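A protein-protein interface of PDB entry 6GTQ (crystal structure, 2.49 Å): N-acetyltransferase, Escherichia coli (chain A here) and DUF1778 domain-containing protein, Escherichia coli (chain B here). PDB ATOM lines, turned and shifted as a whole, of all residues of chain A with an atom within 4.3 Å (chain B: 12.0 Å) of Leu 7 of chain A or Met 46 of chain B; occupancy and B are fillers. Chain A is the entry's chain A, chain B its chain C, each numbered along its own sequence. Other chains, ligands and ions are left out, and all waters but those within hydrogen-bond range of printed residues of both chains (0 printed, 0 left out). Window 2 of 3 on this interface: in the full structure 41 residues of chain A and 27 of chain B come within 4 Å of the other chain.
Leu 7 of chain A touches Met 46 of chain B.
Met 46 of chain B touches Thr 8 of chain A (CE to CA, 3.7 Å).
Ile 9 of chain A touches Leu 43 of chain B (CD1 to CD1, 3.9 Å).
N of Ile 9 of chain A touches CE of Met 46 of chain B, 3.7 Å away.
The backbone NH (N) of Thr 8 of chain A sits at hydrogen-bond distance from the backbone carbonyl oxygen (O) of Cys 53 of chain A (2.8 Å).
No residue of chain B comes within 4 Å of Asp 5 of chain A.
No residue of chain B comes within 4 Å of Asp 6 of chain A.
Printed residues of chain B within 4 Å of Leu 7 of chain A: Met 46 (3.8 Å).
Thr 8 of chain A touches just one residue of chain B: Met 46 (3.7 Å).
Ile 9 of chain A touches just these residues of chain B: Leu 43 (3.9 Å) and Met 46 (3.7 Å).
No residue of chain B comes within 4 Å of Leu 52 of chain A.
No residue of chain B comes within 4 Å of Cys 53 of chain A.
No residue of chain B comes within 4 Å of Arg 54 of chain A.
No residue of chain B comes within 4 Å of Leu 62 of chain A.
Of the printed residues of chain B, Trp 110 of chain A touches Arg 42.
Arg 38 of chain B touches none of the printed residues of chain A.
Of the printed residues of chain A, Leu 43 of chain B touches Ile 9.
Of chain A, only Leu 7 (3.8 Å), Thr 8 (3.7 Å) and Ile 9 (3.7 Å) come within 4 Å of Met 46 of chain B.
The backbone NH (N) of Trp 110 of chain A lies close to the guanidinium group (NH2) of Arg 42 of chain B (3.2 Å).
Printed residues of chain B that touch a printed residue of chain A: Arg 42, Leu 43 and Met 46.
Hydrophobic or aromatic side chains of chain B that line the printed part of chain A: Leu 43 and Met 46.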
ATOM      1  N   ASP A   5      25.079  32.461 -23.862  1.00  0.00           N
ATOM      2  CA  ASP A   5      24.488  31.308 -24.539  1.00  0.00           C
ATOM      3  C   ASP A   5      23.657  31.724 -25.770  1.00  0.00           C
ATOM      4  O   ASP A   5      23.079  32.818 -25.788  1.00  0.00           O
ATOM      5  CB  ASP A   5      23.633  30.474 -23.557  1.00  0.00           C
ATOM      6  CG  ASP A   5      23.777  28.963 -23.699  1.00  0.00           C
ATOM      7  OD1 ASP A   5      23.623  28.453 -24.834  1.00  0.00           O
ATOM      8  OD2 ASP A   5      24.024  28.293 -22.673  1.00  0.00           O
ATOM      9  N   ASP A   6      23.590  30.830 -26.786  1.00  0.00           N
ATOM     10  CA  ASP A   6      22.857  31.024 -28.047  1.00  0.00           C
ATOM     11  C   ASP A   6      21.342  30.716 -27.921  1.00  0.00           C
ATOM     12  O   ASP A   6      20.559  31.217 -28.718  1.00  0.00           O
ATOM     13  CB  ASP A   6      23.504  30.168 -29.163  1.00  0.00           C
ATOM     14  CG  ASP A   6      23.190  30.547 -30.608  1.00  0.00           C
ATOM     15  OD1 ASP A   6      23.117  31.763 -30.907  1.00  0.00           O
ATOM     16  OD2 ASP A   6      23.056  29.626 -31.446  1.00  0.00           O
ATOM     17  N   LEU A   7      20.941  29.916 -26.913  1.00  0.00           N
ATOM     18  CA  LEU A   7      19.556  29.498 -26.679  1.00  0.00           C
ATOM     19  C   LEU A   7      18.643  30.543 -26.026  1.00  0.00           C
ATOM     20  O   LEU A   7      19.097  31.315 -25.178  1.00  0.00           O
ATOM     21  CB  LEU A   7      19.523  28.204 -25.849  1.00  0.00           C
ATOM     22  CG  LEU A   7      20.032  26.936 -26.535  1.00  0.00           C
ATOM     23  CD1 LEU A   7      20.710  26.034 -25.544  1.00  0.00           C
ATOM     24  CD2 LEU A   7      18.905  26.196 -27.244  1.00  0.00           C
ATOM     25  N   THR A   8      17.342  30.542 -26.414  1.00  0.00           N
ATOM     26  CA  THR A   8      16.280  31.406 -25.859  1.00  0.00           C
ATOM     27  C   THR A   8      14.978  30.623 -25.627  1.00  0.00           C
ATOM     28  O   THR A   8      14.730  29.634 -26.316  1.00  0.00           O
ATOM     29  CB  THR A   8      15.973  32.632 -26.748  1.00  0.00           C
ATOM     30  OG1 THR A   8      15.611  32.208 -28.059  1.00  0.00           O
ATOM     31  CG2 THR A   8      17.107  33.643 -26.797  1.00  0.00           C
ATOM     32  N   ILE A   9      14.147  31.076 -24.659  1.00  0.00           N
ATOM     33  CA  ILE A   9      12.817  30.505 -24.391  1.00  0.00           C
ATOM     34  C   ILE A   9      11.789  31.559 -24.773  1.00  0.00           C
ATOM     35  O   ILE A   9      11.816  32.675 -24.250  1.00  0.00           O
ATOM     36  CB  ILE A   9      12.564  29.961 -22.957  1.00  0.00           C
ATOM     37  CG1 ILE A   9      13.720  29.076 -22.456  1.00  0.00           C
ATOM     38  CG2 ILE A   9      11.223  29.206 -22.912  1.00  0.00           C
ATOM     39  CD1 ILE A   9      13.846  28.990 -20.929  1.00  0.00           C
ATOM     40  N   LEU A  52      12.179  26.215 -26.699  1.00  0.00           N
ATOM     41  CA  LEU A  52      13.586  26.429 -26.362  1.00  0.00           C
ATOM     42  C   LEU A  52      14.305  26.273 -27.706  1.00  0.00           C
ATOM     43  O   LEU A  52      14.284  25.186 -28.277  1.00  0.00           O
ATOM     44  CB  LEU A  52      14.085  25.381 -25.343  1.00  0.00           C
ATOM     45  CG  LEU A  52      15.589  25.388 -25.006  1.00  0.00           C
ATOM     46  CD1 LEU A  52      15.985  26.622 -24.213  1.00  0.00           C
ATOM     47  CD2 LEU A  52      15.991  24.124 -24.283  1.00  0.00           C
ATOM     48  N   CYS A  53      14.844  27.367 -28.257  1.00  0.00           N
ATOM     49  CA  CYS A  53      15.505  27.325 -29.562  1.00  0.00           C
ATOM     50  C   CYS A  53      16.833  28.075 -29.586  1.00  0.00           C
ATOM     51  O   CYS A  53      17.164  28.778 -28.632  1.00  0.00           O
ATOM     52  CB  CYS A  53      14.572  27.772 -30.690  1.00  0.00           C
ATOM     53  SG  CYS A  53      13.837  29.407 -30.451  1.00  0.00           S
ATOM     54  N   ARG A  54      17.590  27.896 -30.689  1.00  0.00           N
ATOM     55  CA  ARG A  54      18.935  28.405 -30.934  1.00  0.00           C
ATOM     56  C   ARG A  54      19.068  29.921 -31.254  1.00  0.00           C
ATOM     57  O   ARG A  54      20.197  30.357 -31.493  1.00  0.00           O
ATOM     58  CB  ARG A  54      19.589  27.574 -32.053  1.00  0.00           C
ATOM     59  CG  ARG A  54      20.925  26.954 -31.656  1.00  0.00           C
ATOM     60  N   LEU A  62      15.189  22.925 -29.623  1.00  0.00           N
ATOM     61  CA  LEU A  62      15.934  21.967 -28.807  1.00  0.00           C
ATOM     62  C   LEU A  62      15.219  21.633 -27.486  1.00  0.00           C
ATOM     63  O   LEU A  62      15.829  21.135 -26.541  1.00  0.00           O
ATOM     64  CB  LEU A  62      17.389  22.437 -28.577  1.00  0.00           C
ATOM     65  CG  LEU A  62      18.316  22.446 -29.812  1.00  0.00           C
ATOM     66  CD1 LEU A  62      19.620  23.122 -29.498  1.00  0.00           C
ATOM     67  CD2 LEU A  62      18.561  21.045 -30.355  1.00  0.00           C
ATOM     68  N   LEU A 105      21.022  18.410 -25.502  1.00  0.00           N
ATOM     69  CA  LEU A 105      21.059  19.331 -24.365  1.00  0.00           C
ATOM     70  C   LEU A 105      20.959  18.654 -23.000  1.00  0.00           C
ATOM     71  O   LEU A 105      21.325  19.272 -21.995  1.00  0.00           O
ATOM     72  CB  LEU A 105      19.985  20.421 -24.505  1.00  0.00           C
ATOM     73  CG  LEU A 105      20.259  21.532 -25.525  1.00  0.00           C
ATOM     74  CD1 LEU A 105      19.231  22.614 -25.402  1.00  0.00           C
ATOM     75  CD2 LEU A 105      21.646  22.156 -25.337  1.00  0.00           C
ATOM     76  N   TRP A 110      18.313  21.936 -18.631  1.00  0.00           N
ATOM     77  CA  TRP A 110      17.356  22.691 -19.450  1.00  0.00           C
ATOM     78  C   TRP A 110      15.898  22.388 -19.138  1.00  0.00           C
ATOM     79  O   TRP A 110      15.060  23.280 -19.285  1.00  0.00           O
ATOM     80  CB  TRP A 110      17.646  22.547 -20.950  1.00  0.00           C
ATOM     81  CG  TRP A 110      18.850  23.347 -21.345  1.00  0.00           C
ATOM     82  CD1 TRP A 110      20.106  22.875 -21.582  1.00  0.00           C
ATOM     83  CD2 TRP A 110      18.947  24.781 -21.376  1.00  0.00           C
ATOM     84  NE1 TRP A 110      20.969  23.921 -21.814  1.00  0.00           N
ATOM     85  CE2 TRP A 110      20.287  25.103 -21.681  1.00  0.00           C
ATOM     86  CE3 TRP A 110      18.027  25.825 -21.178  1.00  0.00           C
ATOM     87  CZ2 TRP A 110      20.727  26.425 -21.812  1.00  0.00           C
ATOM     88  CZ3 TRP A 110      18.462  27.134 -21.304  1.00  0.00           C
ATOM     89  CH2 TRP A 110      19.797  27.425 -21.614  1.00  0.00           C
ATOM     90  N   LEU B  36      15.720  23.959  -8.078  1.00  0.00           N
ATOM     91  CA  LEU B  36      14.806  24.934  -8.660  1.00  0.00           C
ATOM     92  C   LEU B  36      15.373  26.356  -8.622  1.00  0.00           C
ATOM     93  O   LEU B  36      15.140  27.126  -9.560  1.00  0.00           O
ATOM     94  CB  LEU B  36      13.441  24.862  -7.957  1.00  0.00           C
ATOM     95  CG  LEU B  36      12.258  25.524  -8.677  1.00  0.00           C
ATOM     96  CD1 LEU B  36      11.998  24.899 -10.048  1.00  0.00           C
ATOM     97  CD2 LEU B  36      11.027  25.449  -7.838  1.00  0.00           C
ATOM     98  N   LYS B  37      16.098  26.707  -7.542  1.00  0.00           N
ATOM     99  CA  LYS B  37      16.744  28.018  -7.378  1.00  0.00           C
ATOM    100  C   LYS B  37      17.814  28.226  -8.458  1.00  0.00           C
ATOM    101  O   LYS B  37      17.914  29.325  -9.014  1.00  0.00           O
ATOM    102  CB  LYS B  37      17.340  28.168  -5.969  1.00  0.00           C
ATOM    103  CG  LYS B  37      16.309  28.580  -4.909  1.00  0.00           C
ATOM    104  CD  LYS B  37      16.777  28.300  -3.469  1.00  0.00           C
ATOM    105  CE  LYS B  37      17.636  29.395  -2.875  1.00  0.00           C
ATOM    106  NZ  LYS B  37      18.177  29.013  -1.543  1.00  0.00           N
ATOM    107  N   ARG B  38      18.567  27.150  -8.785  1.00  0.00           N
ATOM    108  CA  ARG B  38      19.598  27.120  -9.827  1.00  0.00           C
ATOM    109  C   ARG B  38      18.961  27.410 -11.186  1.00  0.00           C
ATOM    110  O   ARG B  38      19.456  28.267 -11.922  1.00  0.00           O
ATOM    111  CB  ARG B  38      20.279  25.744  -9.871  1.00  0.00           C
ATOM    112  CG  ARG B  38      21.405  25.555  -8.866  1.00  0.00           C
ATOM    113  CD  ARG B  38      22.239  24.321  -9.189  1.00  0.00           C
ATOM    114  NE  ARG B  38      21.567  23.057  -8.859  1.00  0.00           N
ATOM    115  CZ  ARG B  38      21.598  22.477  -7.660  1.00  0.00           C
ATOM    116  NH1 ARG B  38      22.249  23.047  -6.652  1.00  0.00           N
ATOM    117  NH2 ARG B  38      20.972  21.324  -7.458  1.00  0.00           N
ATOM    118  N   ALA B  39      17.854  26.697 -11.498  1.00  0.00           N
ATOM    119  CA  ALA B  39      17.066  26.839 -12.724  1.00  0.00           C
ATOM    120  C   ALA B  39      16.577  28.281 -12.883  1.00  0.00           C
ATOM    121  O   ALA B  39      16.711  28.845 -13.967  1.00  0.00           O
ATOM    122  CB  ALA B  39      15.886  25.884 -12.690  1.00  0.00           C
ATOM    123  N   ALA B  40      16.074  28.888 -11.784  1.00  0.00           N
ATOM    124  CA  ALA B  40      15.582  30.273 -11.741  1.00  0.00           C
ATOM    125  C   ALA B  40      16.688  31.310 -12.002  1.00  0.00           C
ATOM    126  O   ALA B  40      16.418  32.322 -12.655  1.00  0.00           O
ATOM    127  CB  ALA B  40      14.907  30.554 -10.404  1.00  0.00           C
ATOM    128  N   LYS B  41      17.914  31.059 -11.484  1.00  0.00           N
ATOM    129  CA  LYS B  41      19.086  31.926 -11.653  1.00  0.00           C
ATOM    130  C   LYS B  41      19.620  31.838 -13.094  1.00  0.00           C
ATOM    131  O   LYS B  41      20.092  32.839 -13.639  1.00  0.00           O
ATOM    132  CB  LYS B  41      20.182  31.564 -10.634  1.00  0.00           C
ATOM    133  CG  LYS B  41      21.133  32.712 -10.296  1.00  0.00           C
ATOM    134  CD  LYS B  41      22.486  32.554 -10.989  1.00  0.00           C
ATOM    135  CE  LYS B  41      23.378  33.762 -10.822  1.00  0.00           C
ATOM    136  NZ  LYS B  41      24.586  33.670 -11.680  1.00  0.00           N
ATOM    137  N   ARG B  42      19.514  30.642 -13.709  1.00  0.00           N
ATOM    138  CA  ARG B  42      19.926  30.368 -15.090  1.00  0.00           C
ATOM    139  C   ARG B  42      19.010  31.080 -16.075  1.00  0.00           C
ATOM    140  O   ARG B  42      19.466  31.552 -17.117  1.00  0.00           O
ATOM    141  CB  ARG B  42      19.894  28.866 -15.360  1.00  0.00           C
ATOM    142  CG  ARG B  42      20.930  28.458 -16.374  1.00  0.00           C
ATOM    143  CD  ARG B  42      21.462  27.083 -16.070  1.00  0.00           C
ATOM    144  NE  ARG B  42      20.635  26.055 -16.693  1.00  0.00           N
ATOM    145  CZ  ARG B  42      20.834  25.579 -17.915  1.00  0.00           C
ATOM    146  NH1 ARG B  42      21.851  26.017 -18.648  1.00  0.00           N
ATOM    147  NH2 ARG B  42      20.033  24.647 -18.408  1.00  0.00           N
ATOM    148  N   LEU B  43      17.716  31.137 -15.727  1.00  0.00           N
ATOM    149  CA  LEU B  43      16.645  31.775 -16.477  1.00  0.00           C
ATOM    150  C   LEU B  43      16.756  33.305 -16.391  1.00  0.00           C
ATOM    151  O   LEU B  43      16.550  33.980 -17.401  1.00  0.00           O
ATOM    152  CB  LEU B  43      15.293  31.286 -15.919  1.00  0.00           C
ATOM    153  CG  LEU B  43      14.019  31.910 -16.476  1.00  0.00           C
ATOM    154  CD1 LEU B  43      13.705  31.370 -17.864  1.00  0.00           C
ATOM    155  CD2 LEU B  43      12.854  31.710 -15.512  1.00  0.00           C
ATOM    156  N   GLN B  44      17.073  33.838 -15.189  1.00  0.00           N
ATOM    157  CA  GLN B  44      17.215  35.270 -14.891  1.00  0.00           C
ATOM    158  C   GLN B  44      18.057  35.981 -15.953  1.00  0.00           C
ATOM    159  O   GLN B  44      17.520  36.785 -16.720  1.00  0.00           O
ATOM    160  CB  GLN B  44      17.788  35.470 -13.475  1.00  0.00           C
ATOM    161  CG  GLN B  44      17.626  36.883 -12.930  1.00  0.00           C
ATOM    162  CD  GLN B  44      18.143  36.996 -11.521  1.00  0.00           C
ATOM    163  OE1 GLN B  44      17.386  36.897 -10.548  1.00  0.00           O
ATOM    164  NE2 GLN B  44      19.447  37.206 -11.377  1.00  0.00           N
ATOM    165  N   GLY B  45      19.338  35.627 -16.027  1.00  0.00           N
ATOM    166  CA  GLY B  45      20.263  36.167 -17.011  1.00  0.00           C
ATOM    167  C   GLY B  45      20.393  35.209 -18.172  1.00  0.00           C
ATOM    168  O   GLY B  45      21.150  34.235 -18.085  1.00  0.00           O
ATOM    169  N   MET B  46      19.626  35.454 -19.254  1.00  0.00           N
ATOM    170  CA  MET B  46      19.635  34.596 -20.436  1.00  0.00           C
ATOM    171  C   MET B  46      19.754  35.378 -21.737  1.00  0.00           C
ATOM    172  O   MET B  46      20.569  35.026 -22.589  1.00  0.00           O
ATOM    173  CB  MET B  46      18.411  33.673 -20.451  1.00  0.00           C
ATOM    174  CG  MET B  46      18.783  32.207 -20.508  1.00  0.00           C
ATOM    175  SD  MET B  46      17.374  31.078 -20.523  1.00  0.00           S
ATOM    176  CE  MET B  46      16.834  31.267 -22.179  1.00  0.00           C
